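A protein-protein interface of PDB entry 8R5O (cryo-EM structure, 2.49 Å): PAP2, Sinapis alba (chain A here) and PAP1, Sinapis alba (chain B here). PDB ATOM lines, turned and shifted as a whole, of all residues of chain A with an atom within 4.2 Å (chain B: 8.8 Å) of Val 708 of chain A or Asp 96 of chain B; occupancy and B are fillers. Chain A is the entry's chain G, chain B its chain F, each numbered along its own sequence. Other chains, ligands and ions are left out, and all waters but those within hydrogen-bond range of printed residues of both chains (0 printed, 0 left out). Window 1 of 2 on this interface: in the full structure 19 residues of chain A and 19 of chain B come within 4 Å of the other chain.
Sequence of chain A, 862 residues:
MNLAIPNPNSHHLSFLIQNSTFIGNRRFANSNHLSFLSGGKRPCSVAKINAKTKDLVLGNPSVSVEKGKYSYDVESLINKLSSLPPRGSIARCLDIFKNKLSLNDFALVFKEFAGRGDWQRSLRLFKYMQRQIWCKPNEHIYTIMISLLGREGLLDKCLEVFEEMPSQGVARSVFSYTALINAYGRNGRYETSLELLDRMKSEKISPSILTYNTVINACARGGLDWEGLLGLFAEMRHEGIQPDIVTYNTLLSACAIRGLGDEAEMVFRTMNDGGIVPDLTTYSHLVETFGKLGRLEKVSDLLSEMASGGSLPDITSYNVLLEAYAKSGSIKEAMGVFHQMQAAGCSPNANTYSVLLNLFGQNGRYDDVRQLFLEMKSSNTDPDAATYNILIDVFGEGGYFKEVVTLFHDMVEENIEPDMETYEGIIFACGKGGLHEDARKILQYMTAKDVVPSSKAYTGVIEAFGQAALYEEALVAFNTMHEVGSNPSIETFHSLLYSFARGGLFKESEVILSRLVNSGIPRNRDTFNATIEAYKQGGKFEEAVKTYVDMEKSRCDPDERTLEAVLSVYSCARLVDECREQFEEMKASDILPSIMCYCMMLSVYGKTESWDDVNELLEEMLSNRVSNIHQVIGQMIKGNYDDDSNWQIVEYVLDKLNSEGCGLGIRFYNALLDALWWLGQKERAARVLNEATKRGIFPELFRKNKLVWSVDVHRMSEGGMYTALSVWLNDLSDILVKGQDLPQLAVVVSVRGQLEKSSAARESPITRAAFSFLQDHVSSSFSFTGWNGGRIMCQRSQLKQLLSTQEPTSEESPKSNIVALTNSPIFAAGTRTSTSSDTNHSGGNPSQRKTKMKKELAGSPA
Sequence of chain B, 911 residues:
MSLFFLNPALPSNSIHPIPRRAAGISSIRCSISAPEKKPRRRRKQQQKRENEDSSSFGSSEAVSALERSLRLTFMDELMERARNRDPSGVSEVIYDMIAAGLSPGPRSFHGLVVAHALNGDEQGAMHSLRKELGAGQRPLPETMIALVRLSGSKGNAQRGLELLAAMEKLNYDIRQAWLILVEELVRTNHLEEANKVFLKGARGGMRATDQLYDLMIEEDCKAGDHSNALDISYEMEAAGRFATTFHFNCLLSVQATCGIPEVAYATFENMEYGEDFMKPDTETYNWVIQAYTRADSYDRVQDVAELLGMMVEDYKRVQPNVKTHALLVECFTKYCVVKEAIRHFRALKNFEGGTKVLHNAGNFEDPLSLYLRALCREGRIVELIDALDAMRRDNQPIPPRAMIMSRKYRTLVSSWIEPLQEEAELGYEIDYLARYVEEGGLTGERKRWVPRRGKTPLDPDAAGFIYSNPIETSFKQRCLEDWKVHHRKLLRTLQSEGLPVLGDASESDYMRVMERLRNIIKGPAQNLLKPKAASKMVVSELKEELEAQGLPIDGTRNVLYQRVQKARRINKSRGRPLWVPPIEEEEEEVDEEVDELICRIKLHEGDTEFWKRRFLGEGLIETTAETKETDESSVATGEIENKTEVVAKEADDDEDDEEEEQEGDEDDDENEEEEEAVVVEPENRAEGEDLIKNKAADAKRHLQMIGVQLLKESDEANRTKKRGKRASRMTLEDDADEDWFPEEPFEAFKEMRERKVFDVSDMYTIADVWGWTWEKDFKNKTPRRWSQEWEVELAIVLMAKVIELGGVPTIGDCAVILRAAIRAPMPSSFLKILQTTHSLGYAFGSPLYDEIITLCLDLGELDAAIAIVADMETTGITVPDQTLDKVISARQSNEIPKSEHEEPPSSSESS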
ATOM      1  N   ARG A 703     -12.262  24.993 -22.414  1.00  0.00           N
ATOM      2  CA  ARG A 703     -11.066  25.439 -21.711  1.00  0.00           C
ATOM      3  C   ARG A 703     -10.411  24.217 -21.090  1.00  0.00           C
ATOM      4  O   ARG A 703     -11.082  23.425 -20.422  1.00  0.00           O
ATOM      5  CB  ARG A 703     -11.393  26.467 -20.622  1.00  0.00           C
ATOM      6  CG  ARG A 703     -12.196  27.662 -21.094  1.00  0.00           C
ATOM      7  CD  ARG A 703     -12.439  28.635 -19.952  1.00  0.00           C
ATOM      8  NE  ARG A 703     -11.191  29.180 -19.433  1.00  0.00           N
ATOM      9  CZ  ARG A 703     -10.626  30.298 -19.867  1.00  0.00           C
ATOM     10  NH1 ARG A 703     -11.182  31.029 -20.818  1.00  0.00           N
ATOM     11  NH2 ARG A 703      -9.474  30.693 -19.332  1.00  0.00           N
ATOM     12  N   LYS A 704      -9.104  24.059 -21.307  1.00  0.00           N
ATOM     13  CA  LYS A 704      -8.370  22.893 -20.804  1.00  0.00           C
ATOM     14  C   LYS A 704      -7.037  23.373 -20.237  1.00  0.00           C
ATOM     15  O   LYS A 704      -6.037  23.456 -20.955  1.00  0.00           O
ATOM     16  CB  LYS A 704      -8.172  21.850 -21.897  1.00  0.00           C
ATOM     17  CG  LYS A 704      -9.455  21.402 -22.577  1.00  0.00           C
ATOM     18  CD  LYS A 704      -9.188  20.354 -23.641  1.00  0.00           C
ATOM     19  CE  LYS A 704     -10.336  20.278 -24.631  1.00  0.00           C
ATOM     20  NZ  LYS A 704     -11.646  20.115 -23.950  1.00  0.00           N
ATOM     21  N   ASN A 705      -7.028  23.684 -18.942  1.00  0.00           N
ATOM     22  CA  ASN A 705      -5.794  24.033 -18.249  1.00  0.00           C
ATOM     23  C   ASN A 705      -5.656  23.207 -16.977  1.00  0.00           C
ATOM     24  O   ASN A 705      -6.461  22.304 -16.729  1.00  0.00           O
ATOM     25  CB  ASN A 705      -5.754  25.529 -17.933  1.00  0.00           C
ATOM     26  CG  ASN A 705      -7.017  26.016 -17.258  1.00  0.00           C
ATOM     27  OD1 ASN A 705      -7.151  25.942 -16.038  1.00  0.00           O
ATOM     28  ND2 ASN A 705      -7.954  26.522 -18.051  1.00  0.00           N
ATOM     29  N   LYS A 706      -4.639  23.504 -16.167  1.00  0.00           N
ATOM     30  CA  LYS A 706      -4.422  22.748 -14.939  1.00  0.00           C
ATOM     31  C   LYS A 706      -5.494  23.014 -13.891  1.00  0.00           C
ATOM     32  O   LYS A 706      -5.681  22.187 -12.994  1.00  0.00           O
ATOM     33  CB  LYS A 706      -3.043  23.067 -14.360  1.00  0.00           C
ATOM     34  CG  LYS A 706      -1.887  22.680 -15.268  1.00  0.00           C
ATOM     35  CD  LYS A 706      -0.536  22.876 -14.592  1.00  0.00           C
ATOM     36  CE  LYS A 706      -0.191  21.729 -13.646  1.00  0.00           C
ATOM     37  NZ  LYS A 706      -0.934  21.772 -12.354  1.00  0.00           N
ATOM     38  N   LEU A 707      -6.196  24.141 -13.978  1.00  0.00           N
ATOM     39  CA  LEU A 707      -7.204  24.480 -12.980  1.00  0.00           C
ATOM     40  C   LEU A 707      -8.591  23.974 -13.357  1.00  0.00           C
ATOM     41  O   LEU A 707      -9.252  23.315 -12.550  1.00  0.00           O
ATOM     42  CB  LEU A 707      -7.246  25.996 -12.765  1.00  0.00           C
ATOM     43  CG  LEU A 707      -6.034  26.645 -12.100  1.00  0.00           C
ATOM     44  CD1 LEU A 707      -6.247  28.143 -11.956  1.00  0.00           C
ATOM     45  CD2 LEU A 707      -5.767  26.007 -10.749  1.00  0.00           C
ATOM     46  N   VAL A 708      -9.047  24.273 -14.572  1.00  0.00           N
ATOM     47  CA  VAL A 708     -10.429  24.031 -14.969  1.00  0.00           C
ATOM     48  C   VAL A 708     -10.461  23.324 -16.316  1.00  0.00           C
ATOM     49  O   VAL A 708      -9.740  23.699 -17.247  1.00  0.00           O
ATOM     50  CB  VAL A 708     -11.235  25.345 -15.033  1.00  0.00           C
ATOM     51  CG1 VAL A 708     -12.629  25.095 -15.572  1.00  0.00           C
ATOM     52  CG2 VAL A 708     -11.312  25.987 -13.663  1.00  0.00           C
ATOM     53  N   TRP A 709     -11.298  22.294 -16.411  1.00  0.00           N
ATOM     54  CA  TRP A 709     -11.709  21.691 -17.674  1.00  0.00           C
ATOM     55  C   TRP A 709     -13.193  21.990 -17.842  1.00  0.00           C
ATOM     56  O   TRP A 709     -14.032  21.368 -17.184  1.00  0.00           O
ATOM     57  CB  TRP A 709     -11.447  20.187 -17.678  1.00  0.00           C
ATOM     58  CG  TRP A 709     -10.184  19.784 -18.363  1.00  0.00           C
ATOM     59  CD1 TRP A 709      -8.919  20.178 -18.050  1.00  0.00           C
ATOM     60  CD2 TRP A 709     -10.064  18.885 -19.469  1.00  0.00           C
ATOM     61  NE1 TRP A 709      -8.016  19.588 -18.899  1.00  0.00           N
ATOM     62  CE2 TRP A 709      -8.695  18.788 -19.780  1.00  0.00           C
ATOM     63  CE3 TRP A 709     -10.983  18.156 -20.229  1.00  0.00           C
ATOM     64  CZ2 TRP A 709      -8.221  17.993 -20.820  1.00  0.00           C
ATOM     65  CZ3 TRP A 709     -10.510  17.366 -21.259  1.00  0.00           C
ATOM     66  CH2 TRP A 709      -9.143  17.291 -21.545  1.00  0.00           C
ATOM     67  N   SER A 710     -13.520  22.935 -18.716  1.00  0.00           N
ATOM     68  CA  SER A 710     -14.876  23.452 -18.804  1.00  0.00           C
ATOM     69  C   SER A 710     -15.424  23.320 -20.217  1.00  0.00           C
ATOM     70  O   SER A 710     -14.679  23.344 -21.200  1.00  0.00           O
ATOM     71  CB  SER A 710     -14.940  24.920 -18.372  1.00  0.00           C
ATOM     72  OG  SER A 710     -14.283  25.754 -19.307  1.00  0.00           O
ATOM     73  N   LEU A 745     -10.908  20.680 -11.432  1.00  0.00           N
ATOM     74  CA  LEU A 745     -12.357  20.720 -11.563  1.00  0.00           C
ATOM     75  C   LEU A 745     -12.743  20.498 -13.016  1.00  0.00           C
ATOM     76  O   LEU A 745     -12.042  20.948 -13.924  1.00  0.00           O
ATOM     77  CB  LEU A 745     -12.913  22.064 -11.076  1.00  0.00           C
ATOM     78  CG  LEU A 745     -14.290  21.998 -10.428  1.00  0.00           C
ATOM     79  CD1 LEU A 745     -14.200  21.156  -9.174  1.00  0.00           C
ATOM     80  CD2 LEU A 745     -14.809  23.390 -10.114  1.00  0.00           C
ATOM     81  N   VAL A 747     -16.182  21.305 -15.191  1.00  0.00           N
ATOM     82  CA  VAL A 747     -17.405  22.079 -15.028  1.00  0.00           C
ATOM     83  C   VAL A 747     -18.157  22.140 -16.348  1.00  0.00           C
ATOM     84  O   VAL A 747     -17.570  22.032 -17.430  1.00  0.00           O
ATOM     85  CB  VAL A 747     -17.118  23.510 -14.518  1.00  0.00           C
ATOM     86  CG1 VAL A 747     -18.182  23.943 -13.523  1.00  0.00           C
ATOM     87  CG2 VAL A 747     -15.729  23.601 -13.912  1.00  0.00           C
ATOM     88  N   LEU B  70     -11.188  25.515  -3.242  1.00  0.00           N
ATOM     89  CA  LEU B  70     -10.963  25.964  -4.611  1.00  0.00           C
ATOM     90  C   LEU B  70     -10.443  27.395  -4.649  1.00  0.00           C
ATOM     91  O   LEU B  70      -9.558  27.717  -5.447  1.00  0.00           O
ATOM     92  CB  LEU B  70     -12.249  25.836  -5.425  1.00  0.00           C
ATOM     93  CG  LEU B  70     -12.714  24.410  -5.719  1.00  0.00           C
ATOM     94  CD1 LEU B  70     -13.975  24.422  -6.563  1.00  0.00           C
ATOM     95  CD2 LEU B  70     -11.613  23.625  -6.410  1.00  0.00           C
ATOM     96  N   THR B  73      -6.618  27.519  -4.061  1.00  0.00           N
ATOM     97  CA  THR B  73      -5.777  27.129  -5.186  1.00  0.00           C
ATOM     98  C   THR B  73      -5.956  28.055  -6.384  1.00  0.00           C
ATOM     99  O   THR B  73      -5.032  28.195  -7.192  1.00  0.00           O
ATOM    100  CB  THR B  73      -6.048  25.674  -5.585  1.00  0.00           C
ATOM    101  OG1 THR B  73      -5.167  25.297  -6.650  1.00  0.00           O
ATOM    102  CG2 THR B  73      -7.484  25.483  -6.037  1.00  0.00           C
ATOM    103  N   PHE B  74      -7.122  28.692  -6.517  1.00  0.00           N
ATOM    104  CA  PHE B  74      -7.294  29.690  -7.569  1.00  0.00           C
ATOM    105  C   PHE B  74      -6.543  30.974  -7.237  1.00  0.00           C
ATOM    106  O   PHE B  74      -5.909  31.571  -8.113  1.00  0.00           O
ATOM    107  CB  PHE B  74      -8.777  29.979  -7.792  1.00  0.00           C
ATOM    108  CG  PHE B  74      -9.438  29.054  -8.771  1.00  0.00           C
ATOM    109  CD1 PHE B  74     -10.063  27.899  -8.340  1.00  0.00           C
ATOM    110  CD2 PHE B  74      -9.436  29.340 -10.125  1.00  0.00           C
ATOM    111  CE1 PHE B  74     -10.671  27.048  -9.233  1.00  0.00           C
ATOM    112  CE2 PHE B  74     -10.046  28.493 -11.023  1.00  0.00           C
ATOM    113  CZ  PHE B  74     -10.664  27.345 -10.575  1.00  0.00           C
ATOM    114  N   GLU B  77      -2.706  30.404  -7.694  1.00  0.00           N
ATOM    115  CA  GLU B  77      -2.249  30.543  -9.072  1.00  0.00           C
ATOM    116  C   GLU B  77      -2.297  31.995  -9.528  1.00  0.00           C
ATOM    117  O   GLU B  77      -1.387  32.463 -10.221  1.00  0.00           O
ATOM    118  CB  GLU B  77      -3.090  29.662  -9.994  1.00  0.00           C
ATOM    119  CG  GLU B  77      -2.658  29.700 -11.446  1.00  0.00           C
ATOM    120  CD  GLU B  77      -1.243  29.196 -11.643  1.00  0.00           C
ATOM    121  OE1 GLU B  77      -0.831  28.272 -10.912  1.00  0.00           O
ATOM    122  OE2 GLU B  77      -0.539  29.729 -12.526  1.00  0.00           O
ATOM    123  N   LEU B  78      -3.351  32.721  -9.151  1.00  0.00           N
ATOM    124  CA  LEU B  78      -3.493  34.106  -9.590  1.00  0.00           C
ATOM    125  C   LEU B  78      -2.382  34.979  -9.024  1.00  0.00           C
ATOM    126  O   LEU B  78      -1.758  35.760  -9.751  1.00  0.00           O
ATOM    127  CB  LEU B  78      -4.867  34.642  -9.183  1.00  0.00           C
ATOM    128  CG  LEU B  78      -5.254  36.032  -9.690  1.00  0.00           C
ATOM    129  CD1 LEU B  78      -6.698  36.036 -10.151  1.00  0.00           C
ATOM    130  CD2 LEU B  78      -5.038  37.091  -8.619  1.00  0.00           C
ATOM    131  N   ARG B  81       1.104  34.613 -10.550  1.00  0.00           N
ATOM    132  CA  ARG B  81       1.318  35.240 -11.846  1.00  0.00           C
ATOM    133  C   ARG B  81       1.334  36.757 -11.770  1.00  0.00           C
ATOM    134  O   ARG B  81       1.975  37.402 -12.604  1.00  0.00           O
ATOM    135  CB  ARG B  81       0.244  34.790 -12.842  1.00  0.00           C
ATOM    136  CG  ARG B  81       0.218  33.290 -13.076  1.00  0.00           C
ATOM    137  CD  ARG B  81      -0.805  32.903 -14.127  1.00  0.00           C
ATOM    138  NE  ARG B  81      -0.859  31.461 -14.325  1.00  0.00           N
ATOM    139  CZ  ARG B  81      -1.648  30.850 -15.197  1.00  0.00           C
ATOM    140  NH1 ARG B  81      -2.469  31.529 -15.980  1.00  0.00           N
ATOM    141  NH2 ARG B  81      -1.615  29.524 -15.285  1.00  0.00           N
ATOM    142  N   GLY B  89      -1.587  36.040 -17.783  1.00  0.00           N
ATOM    143  CA  GLY B  89      -1.897  34.863 -16.987  1.00  0.00           C
ATOM    144  C   GLY B  89      -2.912  35.142 -15.895  1.00  0.00           C
ATOM    145  O   GLY B  89      -3.777  34.309 -15.615  1.00  0.00           O
ATOM    146  N   VAL B  90      -2.818  36.313 -15.261  1.00  0.00           N
ATOM    147  CA  VAL B  90      -3.783  36.692 -14.237  1.00  0.00           C
ATOM    148  C   VAL B  90      -5.179  36.838 -14.823  1.00  0.00           C
ATOM    149  O   VAL B  90      -6.173  36.649 -14.116  1.00  0.00           O
ATOM    150  CB  VAL B  90      -3.328  37.992 -13.539  1.00  0.00           C
ATOM    151  CG1 VAL B  90      -4.259  38.351 -12.393  1.00  0.00           C
ATOM    152  CG2 VAL B  90      -1.907  37.847 -13.031  1.00  0.00           C
ATOM    153  N   SER B  91      -5.281  37.150 -16.116  1.00  0.00           N
ATOM    154  CA  SER B  91      -6.590  37.226 -16.753  1.00  0.00           C
ATOM    155  C   SER B  91      -7.155  35.839 -17.028  1.00  0.00           C
ATOM    156  O   SER B  91      -8.372  35.639 -16.963  1.00  0.00           O
ATOM    157  CB  SER B  91      -6.499  38.031 -18.048  1.00  0.00           C
ATOM    158  OG  SER B  91      -6.139  39.377 -17.787  1.00  0.00           O
ATOM    159  N   GLU B  92      -6.288  34.873 -17.340  1.00  0.00           N
ATOM    160  CA  GLU B  92      -6.753  33.515 -17.601  1.00  0.00           C
ATOM    161  C   GLU B  92      -7.355  32.884 -16.353  1.00  0.00           C
ATOM    162  O   GLU B  92      -8.367  32.182 -16.430  1.00  0.00           O
ATOM    163  CB  GLU B  92      -5.602  32.659 -18.130  1.00  0.00           C
ATOM    164  CG  GLU B  92      -4.877  33.251 -19.325  1.00  0.00           C
ATOM    165  CD  GLU B  92      -5.745  33.329 -20.567  1.00  0.00           C
ATOM    166  OE1 GLU B  92      -6.744  32.584 -20.651  1.00  0.00           O
ATOM    167  OE2 GLU B  92      -5.424  34.138 -21.463  1.00  0.00           O
ATOM    168  N   VAL B  93      -6.743  33.124 -15.191  1.00  0.00           N
ATOM    169  CA  VAL B  93      -7.230  32.521 -13.955  1.00  0.00           C
ATOM    170  C   VAL B  93      -8.586  33.100 -13.572  1.00  0.00           C
ATOM    171  O   VAL B  93      -9.456  32.386 -13.060  1.00  0.00           O
ATOM    172  CB  VAL B  93      -6.196  32.702 -12.830  1.00  0.00           C
ATOM    173  CG1 VAL B  93      -6.653  31.991 -11.569  1.00  0.00           C
ATOM    174  CG2 VAL B  93      -4.838  32.186 -13.276  1.00  0.00           C
ATOM    175  N   ILE B  94      -8.788  34.398 -13.807  1.00  0.00           N
ATOM    176  CA  ILE B  94     -10.077  35.011 -13.499  1.00  0.00           C
ATOM    177  C   ILE B  94     -11.182  34.371 -14.330  1.00  0.00           C
ATOM    178  O   ILE B  94     -12.292  34.136 -13.838  1.00  0.00           O
ATOM    179  CB  ILE B  94     -10.013  36.535 -13.714  1.00  0.00           C
ATOM    180  CG1 ILE B  94      -9.045  37.170 -12.716  1.00  0.00           C
ATOM    181  CG2 ILE B  94     -11.391  37.157 -13.573  1.00  0.00           C
ATOM    182  CD1 ILE B  94      -8.975  38.673 -12.806  1.00  0.00           C
ATOM    183  N   TYR B  95     -10.893  34.066 -15.597  1.00  0.00           N
ATOM    184  CA  TYR B  95     -11.870  33.365 -16.423  1.00  0.00           C
ATOM    185  C   TYR B  95     -12.009  31.906 -16.008  1.00  0.00           C
ATOM    186  O   TYR B  95     -13.063  31.300 -16.228  1.00  0.00           O
ATOM    187  CB  TYR B  95     -11.485  33.471 -17.898  1.00  0.00           C
ATOM    188  CG  TYR B  95     -11.642  34.863 -18.459  1.00  0.00           C
ATOM    189  CD1 TYR B  95     -12.730  35.651 -18.113  1.00  0.00           C
ATOM    190  CD2 TYR B  95     -10.696  35.396 -19.324  1.00  0.00           C
ATOM    191  CE1 TYR B  95     -12.879  36.925 -18.619  1.00  0.00           C
ATOM    192  CE2 TYR B  95     -10.836  36.673 -19.835  1.00  0.00           C
ATOM    193  CZ  TYR B  95     -11.930  37.432 -19.479  1.00  0.00           C
ATOM    194  OH  TYR B  95     -12.081  38.704 -19.981  1.00  0.00           O
ATOM    195  N   ASP B  96     -10.961  31.322 -15.424  1.00  0.00           N
ATOM    196  CA  ASP B  96     -11.103  30.008 -14.806  1.00  0.00           C
ATOM    197  C   ASP B  96     -12.036  30.068 -13.604  1.00  0.00           C
ATOM    198  O   ASP B  96     -12.843  29.156 -13.391  1.00  0.00           O
ATOM    199  CB  ASP B  96      -9.734  29.466 -14.396  1.00  0.00           C
ATOM    200  CG  ASP B  96      -8.817  29.242 -15.579  1.00  0.00           C
ATOM    201  OD1 ASP B  96      -9.255  29.466 -16.726  1.00  0.00           O
ATOM    202  OD2 ASP B  96      -7.652  28.845 -15.360  1.00  0.00           O
ATOM    203  N   MET B  97     -11.934  31.132 -12.803  1.00  0.00           N
ATOM    204  CA  MET B  97     -12.847  31.308 -11.679  1.00  0.00           C
ATOM    205  C   MET B  97     -14.283  31.467 -12.155  1.00  0.00           C
ATOM    206  O   MET B  97     -15.213  30.924 -11.548  1.00  0.00           O
ATOM    207  CB  MET B  97     -12.426  32.519 -10.846  1.00  0.00           C
ATOM    208  CG  MET B  97     -11.033  32.421 -10.256  1.00  0.00           C
ATOM    209  SD  MET B  97     -10.474  33.959  -9.504  1.00  0.00           S
ATOM    210  CE  MET B  97     -11.759  34.233  -8.289  1.00  0.00           C
ATOM    211  N   ILE B  98     -14.484  32.220 -13.238  1.00  0.00           N
ATOM    212  CA  ILE B  98     -15.826  32.407 -13.780  1.00  0.00           C
ATOM    213  C   ILE B  98     -16.385  31.085 -14.289  1.00  0.00           C
ATOM    214  O   ILE B  98     -17.572  30.786 -14.108  1.00  0.00           O
ATOM    215  CB  ILE B  98     -15.805  33.484 -14.879  1.00  0.00           C
ATOM    216  CG1 ILE B  98     -15.442  34.844 -14.279  1.00  0.00           C
ATOM    217  CG2 ILE B  98     -17.143  33.555 -15.592  1.00  0.00           C
ATOM    218  CD1 ILE B  98     -15.431  35.972 -15.282  1.00  0.00           C
ATOM    219  N   ALA B  99     -15.542  30.271 -14.930  1.00  0.00           N
ATOM    220  CA  ALA B  99     -15.986  28.962 -15.398  1.00  0.00           C
ATOM    221  C   ALA B  99     -16.396  28.068 -14.235  1.00  0.00           C
ATOM    222  O   ALA B  99     -17.396  27.347 -14.320  1.00  0.00           O
ATOM    223  CB  ALA B  99     -14.883  28.300 -16.223  1.00  0.00           C
ATOM    224  N   ALA B 100     -15.637  28.101 -13.140  1.00  0.00           N
ATOM    225  CA  ALA B 100     -15.982  27.329 -11.953  1.00  0.00           C
ATOM    226  C   ALA B 100     -17.154  27.919 -11.182  1.00  0.00           C
ATOM    227  O   ALA B 100     -17.648  27.271 -10.254  1.00  0.00           O
ATOM    228  CB  ALA B 100     -14.768  27.212 -11.030  1.00  0.00           C
ATOM    229  N   GLY B 101     -17.608  29.118 -11.537  1.00  0.00           N
ATOM    230  CA  GLY B 101     -18.686  29.775 -10.831  1.00  0.00           C
ATOM    231  C   GLY B 101     -18.257  30.658  -9.683  1.00  0.00           C
ATOM    232  O   GLY B 101     -19.107  31.333  -9.090  1.00  0.00           O
ATOM    233  N   LEU B 102     -16.971  30.675  -9.345  1.00  0.00           N
ATOM    234  CA  LEU B 102     -16.482  31.546  -8.287  1.00  0.00           C
ATOM    235  C   LEU B 102     -16.515  33.000  -8.742  1.00  0.00           C
ATOM    236  O   LEU B 102     -16.161  33.321  -9.879  1.00  0.00           O
ATOM    237  CB  LEU B 102     -15.063  31.147  -7.890  1.00  0.00           C
ATOM    238  CG  LEU B 102     -14.885  29.691  -7.455  1.00  0.00           C
ATOM    239  CD1 LEU B 102     -13.415  29.361  -7.269  1.00  0.00           C
ATOM    240  CD2 LEU B 102     -15.664  29.415  -6.179  1.00  0.00           C
ATOM    241  N   SER B 103     -16.946  33.884  -7.845  1.00  0.00           N
ATOM    242  CA  SER B 103     -17.040  35.302  -8.164  1.00  0.00           C
ATOM    243  C   SER B 103     -15.744  36.001  -7.781  1.00  0.00           C
ATOM    244  O   SER B 103     -15.358  35.961  -6.604  1.00  0.00           O
ATOM    245  CB  SER B 103     -18.212  35.942  -7.440  1.00  0.00           C
ATOM    246  OG  SER B 103     -19.441  35.371  -7.856  1.00  0.00           O
ATOM    247  N   PRO B 104     -15.043  36.637  -8.721  1.00  0.00           N
ATOM    248  CA  PRO B 104     -13.787  37.327  -8.384  1.00  0.00           C
ATOM    249  C   PRO B 104     -14.047  38.493  -7.442  1.00  0.00           C
ATOM    250  O   PRO B 104     -14.842  39.387  -7.742  1.00  0.00           O
ATOM    251  CB  PRO B 104     -13.264  37.803  -9.745  1.00  0.00           C
ATOM    252  CG  PRO B 104     -13.990  36.974 -10.757  1.00  0.00           C
ATOM    253  CD  PRO B 104     -15.332  36.694 -10.162  1.00  0.00           C
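Among the printed residues, merely in contact across the chains: Arg 703 of chain A with Tyr 95 of chain B (3.7 Å), Leu 707 of chain A with Phe 74 of chain B (3.9 Å), Leu 707 of chain A with Glu 77 of chain B (3.9 Å), Leu 707 of chain A with Val 93 of chain B (3.9 Å), Leu 707 of chain A with Asp 96 of chain B (3.7 Å), Val 708 of chain A with Phe 74 of chain B (3.4 Å), Val 708 of chain A with Asp 96 of chain B (3.5 Å), Val 708 of chain A with Ala 99 of chain B (3.97 Å), Leu 745 of chain A with Leu 70 of chain B (3.8 Å), Leu 745 of chain A with Ala 100 of chain B (3.9 Å) and Val 747 of chain A with Ala 99 of chain B (3.6 Å).
The side-chain carboxylate (OD2) of Asp 96 of chain B sits close to the side-chain amide oxygen (OD1) of Asn 705 of chain A.
The side-chain carboxylate of Glu 92 of chain B is in salt-bridge range of the guanidinium group of Arg 703 of chain A, 3.6 Å away.
OD1 of Asp 96 of chain B is in salt-bridge range of NH2 of Arg 703 of chain A, at 2.9 Å.
Of the printed residues of chain B, Val 708 of chain A touches Phe 74 (3.4 Å), Asp 96 (3.5 Å) and Ala 99 (3.97 Å).
Asp 96 of chain B touches just these residues of chain A: Arg 703, Asn 705, Leu 707 and Val 708.
Asn 705 of chain A touches just one residue of chain B: Asp 96.
Of the printed residues of chain A, Ala 99 of chain B touches Val 708 and Val 747.
Printed residues of chain B within 4 Å of Leu 745 of chain A: Leu 70 and Ala 100.
Ser 103 of chain B touches none of the printed residues of chain A.
The nearest residue of chain B that does not touch Val 708 of chain A is Ala 100 of chain B (4.5 Å).
The guanidinium group of Arg 81 of chain B is in salt-bridge range of the side-chain carboxylate of Glu 77 of chain B, 2.5 Å away.
The backbone NH of Trp 709 of chain A is in hydrogen-bond range of the backbone carbonyl oxygen of Leu 745 of chain A, at 2.9 Å.
The side-chain amide oxygen (OD1) of Asn 705 of chain A is in hydrogen-bond range of the backbone NH (N) of Val 708 of chain A.
N of Ser 710 of chain A is in hydrogen-bond range of O of Arg 703 of chain A (3.0 Å).
The backbone carbonyl oxygen (O) of Trp 709 of chain A lies within hydrogen-bond range of the backbone NH (N) of Val 747 of chain A (2.9 Å).
O of Leu 707 of chain A is in hydrogen-bond range of N of Leu 745 of chain A, at 3.3 Å.
Of the 10 printed residues of chain A, 6 touch a printed residue of chain B.
Hydrophobic or aromatic side chains of chain A within 4 Å of the printed part of chain B: Leu 707, Val 708, Leu 745 and Val 747.
Among the printed residues, 14 pairs touch across the chains.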
